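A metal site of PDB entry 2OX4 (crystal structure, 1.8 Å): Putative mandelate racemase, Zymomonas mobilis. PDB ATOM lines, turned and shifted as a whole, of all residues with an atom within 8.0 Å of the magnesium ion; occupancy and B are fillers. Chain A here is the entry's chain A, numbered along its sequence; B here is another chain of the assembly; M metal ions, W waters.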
ATOM      1  N   TYR A  44     -34.010 -17.614  20.501  1.00  0.00           N
ATOM      2  CA  TYR A  44     -33.315 -16.611  19.700  1.00  0.00           C
ATOM      3  C   TYR A  44     -33.939 -16.572  18.288  1.00  0.00           C
ATOM      4  O   TYR A  44     -34.806 -17.381  17.975  1.00  0.00           O
ATOM      5  CB  TYR A  44     -31.811 -16.910  19.645  1.00  0.00           C
ATOM      6  CG  TYR A  44     -31.482 -18.292  19.072  1.00  0.00           C
ATOM      7  CD1 TYR A  44     -31.008 -18.424  17.774  1.00  0.00           C
ATOM      8  CD2 TYR A  44     -31.651 -19.458  19.848  1.00  0.00           C
ATOM      9  CE1 TYR A  44     -30.712 -19.682  17.241  1.00  0.00           C
ATOM     10  CE2 TYR A  44     -31.363 -20.721  19.315  1.00  0.00           C
ATOM     11  CZ  TYR A  44     -30.887 -20.816  18.019  1.00  0.00           C
ATOM     12  OH  TYR A  44     -30.588 -22.059  17.493  1.00  0.00           O
ATOM     13  N   TYR A 129     -17.359 -28.395  24.719  1.00  0.00           N
ATOM     14  CA  TYR A 129     -16.718 -27.298  24.012  1.00  0.00           C
ATOM     15  C   TYR A 129     -17.266 -25.925  24.381  1.00  0.00           C
ATOM     16  O   TYR A 129     -18.446 -25.788  24.739  1.00  0.00           O
ATOM     17  CB  TYR A 129     -16.664 -27.530  22.503  1.00  0.00           C
ATOM     18  CG  TYR A 129     -17.940 -27.360  21.703  1.00  0.00           C
ATOM     19  CD1 TYR A 129     -18.411 -26.101  21.320  1.00  0.00           C
ATOM     20  CD2 TYR A 129     -18.643 -28.489  21.250  1.00  0.00           C
ATOM     21  CE1 TYR A 129     -19.583 -25.962  20.555  1.00  0.00           C
ATOM     22  CE2 TYR A 129     -19.800 -28.356  20.479  1.00  0.00           C
ATOM     23  CZ  TYR A 129     -20.248 -27.101  20.122  1.00  0.00           C
ATOM     24  OH  TYR A 129     -21.388 -26.980  19.357  1.00  0.00           O
ATOM     25  N   SER A 131     -18.580 -22.555  23.225  1.00  0.00           N
ATOM     26  CA  SER A 131     -19.305 -22.257  21.988  1.00  0.00           C
ATOM     27  C   SER A 131     -19.467 -20.761  21.724  1.00  0.00           C
ATOM     28  O   SER A 131     -19.842 -20.008  22.624  1.00  0.00           O
ATOM     29  CB  SER A 131     -20.674 -22.909  22.016  1.00  0.00           C
ATOM     30  OG  SER A 131     -21.273 -22.804  20.740  1.00  0.00           O
ATOM     31  N   GLN A 132     -19.221 -20.376  20.478  1.00  0.00           N
ATOM     32  CA  GLN A 132     -19.485 -19.039  19.939  1.00  0.00           C
ATOM     33  C   GLN A 132     -18.495 -17.992  20.451  1.00  0.00           C
ATOM     34  O   GLN A 132     -18.892 -16.954  20.994  1.00  0.00           O
ATOM     35  CB  GLN A 132     -20.953 -18.569  20.150  1.00  0.00           C
ATOM     36  CG  GLN A 132     -22.052 -19.603  19.823  1.00  0.00           C
ATOM     37  CD  GLN A 132     -22.083 -20.069  18.370  1.00  0.00           C
ATOM     38  OE1 GLN A 132     -21.373 -19.541  17.510  1.00  0.00           O
ATOM     39  NE2 GLN A 132     -22.907 -21.076  18.097  1.00  0.00           N
ATOM     40  N   LYS A 166     -15.714 -23.571  19.604  1.00  0.00           N
ATOM     41  CA  LYS A 166     -16.441 -23.335  18.358  1.00  0.00           C
ATOM     42  C   LYS A 166     -16.541 -21.863  18.028  1.00  0.00           C
ATOM     43  O   LYS A 166     -16.799 -21.025  18.899  1.00  0.00           O
ATOM     44  CB  LYS A 166     -17.842 -23.967  18.387  1.00  0.00           C
ATOM     45  CG  LYS A 166     -18.638 -23.785  17.079  1.00  0.00           C
ATOM     46  CD  LYS A 166     -19.916 -24.669  17.070  1.00  0.00           C
ATOM     47  CE  LYS A 166     -21.113 -23.920  17.634  1.00  0.00           C
ATOM     48  NZ  LYS A 166     -22.307 -24.811  17.768  1.00  0.00           N
ATOM     49  N   GLU A 215     -18.447 -22.833  12.662  1.00  0.00           N
ATOM     50  CA  GLU A 215     -19.890 -22.635  12.594  1.00  0.00           C
ATOM     51  C   GLU A 215     -20.210 -21.635  11.474  1.00  0.00           C
ATOM     52  O   GLU A 215     -19.735 -20.513  11.523  1.00  0.00           O
ATOM     53  CB  GLU A 215     -20.322 -22.048  13.947  1.00  0.00           C
ATOM     54  CG  GLU A 215     -21.644 -21.285  13.933  1.00  0.00           C
ATOM     55  CD  GLU A 215     -22.834 -22.222  14.025  1.00  0.00           C
ATOM     56  OE1 GLU A 215     -23.316 -22.485  15.149  1.00  0.00           O
ATOM     57  OE2 GLU A 215     -23.275 -22.690  12.966  1.00  0.00           O
ATOM     58  N   ASN A 216     -21.036 -22.002  10.499  1.00  0.00           N
ATOM     59  CA  ASN A 216     -21.397 -21.062   9.437  1.00  0.00           C
ATOM     60  C   ASN A 216     -22.785 -20.439   9.640  1.00  0.00           C
ATOM     61  O   ASN A 216     -23.151 -19.511   8.922  1.00  0.00           O
ATOM     62  CB  ASN A 216     -21.339 -21.729   8.055  1.00  0.00           C
ATOM     63  CG  ASN A 216     -19.927 -21.828   7.481  1.00  0.00           C
ATOM     64  OD1 ASN A 216     -19.745 -22.173   6.301  1.00  0.00           O
ATOM     65  ND2 ASN A 216     -18.921 -21.569   8.305  1.00  0.00           N
ATOM     66  N   HIS A 217     -23.565 -20.974  10.592  1.00  0.00           N
ATOM     67  CA  HIS A 217     -24.892 -20.429  10.969  1.00  0.00           C
ATOM     68  C   HIS A 217     -25.913 -20.399   9.830  1.00  0.00           C
ATOM     69  O   HIS A 217     -26.851 -19.598   9.847  1.00  0.00           O
ATOM     70  CB  HIS A 217     -24.750 -19.023  11.570  1.00  0.00           C
ATOM     71  CG  HIS A 217     -24.641 -18.993  13.060  1.00  0.00           C
ATOM     72  ND1 HIS A 217     -23.636 -18.321  13.720  1.00  0.00           N
ATOM     73  CD2 HIS A 217     -25.432 -19.530  14.022  1.00  0.00           C
ATOM     74  CE1 HIS A 217     -23.804 -18.451  15.028  1.00  0.00           C
ATOM     75  NE2 HIS A 217     -24.879 -19.191  15.234  1.00  0.00           N
ATOM     76  N   GLY A 218     -25.750 -21.276   8.835  1.00  0.00           N
ATOM     77  CA  GLY A 218     -26.597 -21.248   7.634  1.00  0.00           C
ATOM     78  C   GLY A 218     -26.510 -19.982   6.790  1.00  0.00           C
ATOM     79  O   GLY A 218     -27.394 -19.716   5.967  1.00  0.00           O
ATOM     80  N   GLU A 241     -20.164 -26.794  10.774  1.00  0.00           N
ATOM     81  CA  GLU A 241     -21.574 -26.810  11.196  1.00  0.00           C
ATOM     82  C   GLU A 241     -22.455 -25.857  10.379  1.00  0.00           C
ATOM     83  O   GLU A 241     -22.070 -24.712  10.083  1.00  0.00           O
ATOM     84  CB  GLU A 241     -21.701 -26.479  12.691  1.00  0.00           C
ATOM     85  CG  GLU A 241     -23.123 -26.175  13.155  1.00  0.00           C
ATOM     86  CD  GLU A 241     -23.225 -25.891  14.644  1.00  0.00           C
ATOM     87  OE1 GLU A 241     -22.298 -26.230  15.387  1.00  0.00           O
ATOM     88  OE2 GLU A 241     -24.256 -25.334  15.072  1.00  0.00           O
ATOM     89  N   GLU A 242     -23.658 -26.343  10.037  1.00  0.00           N
ATOM     90  CA  GLU A 242     -24.708 -25.560   9.351  1.00  0.00           C
ATOM     91  C   GLU A 242     -24.194 -24.783   8.151  1.00  0.00           C
ATOM     92  O   GLU A 242     -24.212 -23.550   8.117  1.00  0.00           O
ATOM     93  CB  GLU A 242     -25.447 -24.638  10.335  1.00  0.00           C
ATOM     94  CG  GLU A 242     -26.432 -25.360  11.239  1.00  0.00           C
ATOM     95  CD  GLU A 242     -27.726 -24.568  11.422  1.00  0.00           C
ATOM     96  OE1 GLU A 242     -27.686 -23.543  12.119  1.00  0.00           O
ATOM     97  OE2 GLU A 242     -28.764 -24.951  10.848  1.00  0.00           O
ATOM     98  N   ALA A 264     -21.692 -31.151  10.296  1.00  0.00           N
ATOM     99  CA  ALA A 264     -22.673 -31.192  11.405  1.00  0.00           C
ATOM    100  C   ALA A 264     -23.882 -30.345  11.071  1.00  0.00           C
ATOM    101  O   ALA A 264     -23.762 -29.313  10.389  1.00  0.00           O
ATOM    102  CB  ALA A 264     -22.044 -30.661  12.703  1.00  0.00           C
ATOM    103  N   SER A 265     -25.040 -30.749  11.593  1.00  0.00           N
ATOM    104  CA  SER A 265     -26.282 -29.973  11.457  1.00  0.00           C
ATOM    105  C   SER A 265     -27.338 -30.579  12.364  1.00  0.00           C
ATOM    106  O   SER A 265     -27.277 -31.759  12.686  1.00  0.00           O
ATOM    107  CB  SER A 265     -26.802 -30.043  10.015  1.00  0.00           C
ATOM    108  OG  SER A 265     -27.801 -29.070   9.785  1.00  0.00           O
ATOM    109  N   GLY A 266     -28.315 -29.777  12.779  1.00  0.00           N
ATOM    110  CA  GLY A 266     -29.431 -30.354  13.503  1.00  0.00           C
ATOM    111  C   GLY A 266     -30.352 -29.366  14.168  1.00  0.00           C
ATOM    112  O   GLY A 266     -31.491 -29.712  14.473  1.00  0.00           O
ATOM    113  N   GLU A 267     -29.859 -28.156  14.430  1.00  0.00           N
ATOM    114  CA  GLU A 267     -30.672 -27.236  15.192  1.00  0.00           C
ATOM    115  C   GLU A 267     -31.888 -26.747  14.385  1.00  0.00           C
ATOM    116  O   GLU A 267     -32.849 -26.258  14.965  1.00  0.00           O
ATOM    117  CB  GLU A 267     -29.845 -26.079  15.755  1.00  0.00           C
ATOM    118  CG  GLU A 267     -29.442 -25.070  14.734  1.00  0.00           C
ATOM    119  CD  GLU A 267     -28.346 -24.159  15.233  1.00  0.00           C
ATOM    120  OE1 GLU A 267     -27.183 -24.599  15.271  1.00  0.00           O
ATOM    121  OE2 GLU A 267     -28.665 -23.010  15.599  1.00  0.00           O
ATOM    122  N   ARG A 268     -31.828 -26.884  13.063  1.00  0.00           N
ATOM    123  CA  ARG A 268     -32.958 -26.531  12.208  1.00  0.00           C
ATOM    124  C   ARG A 268     -33.471 -27.742  11.412  1.00  0.00           C
ATOM    125  O   ARG A 268     -33.981 -27.613  10.293  1.00  0.00           O
ATOM    126  CB  ARG A 268     -32.578 -25.344  11.310  1.00  0.00           C
ATOM    127  CG  ARG A 268     -32.581 -24.027  12.081  1.00  0.00           C
ATOM    128  CD  ARG A 268     -32.281 -22.877  11.155  1.00  0.00           C
ATOM    129  NE  ARG A 268     -30.849 -22.793  10.878  1.00  0.00           N
ATOM    130  CZ  ARG A 268     -30.261 -21.710  10.395  1.00  0.00           C
ATOM    131  NH1 ARG A 268     -31.002 -20.621  10.125  1.00  0.00           N
ATOM    132  NH2 ARG A 268     -28.946 -21.713  10.178  1.00  0.00           N
ATOM    133  N   GLN A 288     -27.083 -32.577  15.417  1.00  0.00           N
ATOM    134  CA  GLN A 288     -27.199 -31.632  16.520  1.00  0.00           C
ATOM    135  C   GLN A 288     -28.659 -31.269  16.787  1.00  0.00           C
ATOM    136  O   GLN A 288     -29.012 -30.076  16.825  1.00  0.00           O
ATOM    137  CB  GLN A 288     -26.394 -30.360  16.221  1.00  0.00           C
ATOM    138  CG  GLN A 288     -24.912 -30.589  15.939  1.00  0.00           C
ATOM    139  CD  GLN A 288     -24.243 -29.364  15.335  1.00  0.00           C
ATOM    140  OE1 GLN A 288     -24.720 -28.818  14.348  1.00  0.00           O
ATOM    141  NE2 GLN A 288     -23.138 -28.940  15.932  1.00  0.00           N
ATOM    142  N   GLN A 315     -24.290 -34.309  19.135  1.00  0.00           N
ATOM    143  CA  GLN A 315     -24.065 -33.242  20.117  1.00  0.00           C
ATOM    144  C   GLN A 315     -25.371 -32.479  20.190  1.00  0.00           C
ATOM    145  O   GLN A 315     -25.749 -31.861  19.205  1.00  0.00           O
ATOM    146  CB  GLN A 315     -22.984 -32.298  19.588  1.00  0.00           C
ATOM    147  CG  GLN A 315     -22.867 -30.928  20.338  1.00  0.00           C
ATOM    148  CD  GLN A 315     -22.999 -29.773  19.416  1.00  0.00           C
ATOM    149  OE1 GLN A 315     -22.122 -29.506  18.602  1.00  0.00           O
ATOM    150  NE2 GLN A 315     -24.107 -29.048  19.533  1.00  0.00           N
ATOM    151  N   HIS A 317     -27.933 -29.667  20.405  1.00  0.00           N
ATOM    152  CA  HIS A 317     -27.849 -28.228  20.272  1.00  0.00           C
ATOM    153  C   HIS A 317     -28.436 -27.614  21.548  1.00  0.00           C
ATOM    154  O   HIS A 317     -29.552 -27.954  21.949  1.00  0.00           O
ATOM    155  CB  HIS A 317     -28.660 -27.749  19.083  1.00  0.00           C
ATOM    156  CG  HIS A 317     -28.714 -26.266  18.976  1.00  0.00           C
ATOM    157  ND1 HIS A 317     -29.783 -25.531  19.441  1.00  0.00           N
ATOM    158  CD2 HIS A 317     -27.822 -25.378  18.497  1.00  0.00           C
ATOM    159  CE1 HIS A 317     -29.547 -24.244  19.244  1.00  0.00           C
ATOM    160  NE2 HIS A 317     -28.364 -24.121  18.674  1.00  0.00           N
ATOM    161  N   VAL A 318     -27.657 -26.745  22.197  1.00  0.00           N
ATOM    162  CA  VAL A 318     -28.076 -26.195  23.486  1.00  0.00           C
ATOM    163  C   VAL A 318     -27.853 -24.689  23.457  1.00  0.00           C
ATOM    164  O   VAL A 318     -26.710 -24.229  23.398  1.00  0.00           O
ATOM    165  CB  VAL A 318     -27.298 -26.805  24.677  1.00  0.00           C
ATOM    166  CG1 VAL A 318     -27.830 -26.263  26.011  1.00  0.00           C
ATOM    167  CG2 VAL A 318     -27.381 -28.314  24.660  1.00  0.00           C
ATOM    168  N   ALA A 319     -28.939 -23.935  23.520  1.00  0.00           N
ATOM    169  CA  ALA A 319     -28.879 -22.475  23.418  1.00  0.00           C
ATOM    170  C   ALA A 319     -30.136 -21.804  23.978  1.00  0.00           C
ATOM    171  O   ALA A 319     -30.802 -21.037  23.261  1.00  0.00           O
ATOM    172  CB  ALA A 319     -28.658 -22.055  21.952  1.00  0.00           C
ATOM    173  N   GLU A 342     -22.112 -28.882  23.771  1.00  0.00           N
ATOM    174  CA  GLU A 342     -22.033 -27.456  23.493  1.00  0.00           C
ATOM    175  C   GLU A 342     -22.320 -26.638  24.759  1.00  0.00           C
ATOM    176  O   GLU A 342     -23.419 -26.707  25.333  1.00  0.00           O
ATOM    177  CB  GLU A 342     -23.059 -27.077  22.401  1.00  0.00           C
ATOM    178  CG  GLU A 342     -23.153 -25.588  22.193  1.00  0.00           C
ATOM    179  CD  GLU A 342     -23.989 -25.194  20.997  1.00  0.00           C
ATOM    180  OE1 GLU A 342     -24.967 -25.894  20.650  1.00  0.00           O
ATOM    181  OE2 GLU A 342     -23.674 -24.138  20.417  1.00  0.00           O
ATOM    182  N   HIS A 344     -22.673 -22.888  25.671  1.00  0.00           N
ATOM    183  CA  HIS A 344     -22.885 -21.613  24.999  1.00  0.00           C
ATOM    184  C   HIS A 344     -22.475 -20.482  25.928  1.00  0.00           C
ATOM    185  O   HIS A 344     -22.689 -20.557  27.153  1.00  0.00           O
ATOM    186  CB  HIS A 344     -24.350 -21.458  24.604  1.00  0.00           C
ATOM    187  CG  HIS A 344     -24.575 -20.549  23.449  1.00  0.00           C
ATOM    188  ND1 HIS A 344     -24.409 -19.187  23.534  1.00  0.00           N
ATOM    189  CD2 HIS A 344     -24.966 -20.803  22.175  1.00  0.00           C
ATOM    190  CE1 HIS A 344     -24.675 -18.630  22.354  1.00  0.00           C
ATOM    191  NE2 HIS A 344     -25.018 -19.596  21.516  1.00  0.00           N
ATOM    192  N   PHE B  82     -33.859 -16.646  11.082  1.00  0.00           N
ATOM    193  CA  PHE B  82     -33.255 -17.910  11.531  1.00  0.00           C
ATOM    194  C   PHE B  82     -34.140 -19.130  11.305  1.00  0.00           C
ATOM    195  O   PHE B  82     -33.720 -20.093  10.667  1.00  0.00           O
ATOM    196  CB  PHE B  82     -32.717 -17.875  12.984  1.00  0.00           C
ATOM    197  CG  PHE B  82     -31.655 -18.910  13.249  1.00  0.00           C
ATOM    198  CD1 PHE B  82     -30.343 -18.685  12.836  1.00  0.00           C
ATOM    199  CD2 PHE B  82     -31.976 -20.127  13.842  1.00  0.00           C
ATOM    200  CE1 PHE B  82     -29.339 -19.644  13.063  1.00  0.00           C
ATOM    201  CE2 PHE B  82     -30.987 -21.100  14.049  1.00  0.00           C
ATOM    202  CZ  PHE B  82     -29.676 -20.856  13.663  1.00  0.00           C
HETATM  203 MG    MG M   1     -25.393 -23.598  15.503  1.00  0.00          MG
HETATM  204  O   HOH W   1     -26.530 -21.623  16.110  1.00  0.00           O
HETATM  205  O   HOH W   2     -25.731 -22.884  13.527  1.00  0.00           O
HETATM  206  O   HOH W   3     -25.037 -23.699  17.670  1.00  0.00           O
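The magnesium ion is bound by the side-chain carboxylate (OE1) of Glu 267, the side-chain carboxylate (OE2) of Glu 241, water W2, water W3, water W1 and the side-chain carboxylate (OE1) of Glu 215.
The backbone NH (N) of Glu 267 lies within hydrogen-bond range of the backbone carbonyl oxygen (O) of Gln 288. The side-chain carboxylate of Glu 241 is in hydrogen-bond range of the side-chain amide nitrogen of Gln 288. O of Glu 241 is in hydrogen-bond range of N of Asn 216. OE1 of Glu 241 lies within salt-bridge range of NZ of Lys 166, 2.8 Å away. The side-chain carboxylate (OE2) of Glu 215 sits at hydrogen-bond distance from the backbone NH (N) of His 217 (2.9 Å). A ring nitrogen (NE2) of His 317 sits at hydrogen-bond distance from the side-chain carboxylate of Glu 267, at 3.3 Å. The side-chain carboxylate (OE2) of Glu 267 lies within hydrogen-bond range of the side-chain hydroxyl (OH) of Tyr 44, at 2.9 Å. The side-chain carboxylate (OE1) of Glu 215 lies close to the side-chain amide nitrogen (NE2) of Gln 132.
Water W3 lies within hydrogen-bond range of the side-chain amino group of Lys 166 (2.9 Å), the side-chain carboxylate of Glu 342 (3.1 Å) and the side-chain amide nitrogen of Gln 132 (3.4 Å). Water W2 lies within hydrogen-bond range of OE1 of Glu 242 (2.5 Å) and OE2 of Glu 215 (2.5 Å). Water W1 bridges the side-chain carboxylate (OE2) of Glu 267 (2.6 Å) and a ring nitrogen (NE2) of His 217 (3.1 Å).
Of the 24 residues printed, 3 come within 4 Å of the magnesium ion. Along chain A the residues within 4 Å of the magnesium ion span positions 215 to 267. The nearest printed residue that does not touch the magnesium ion is Lys 166 (4.02 Å).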
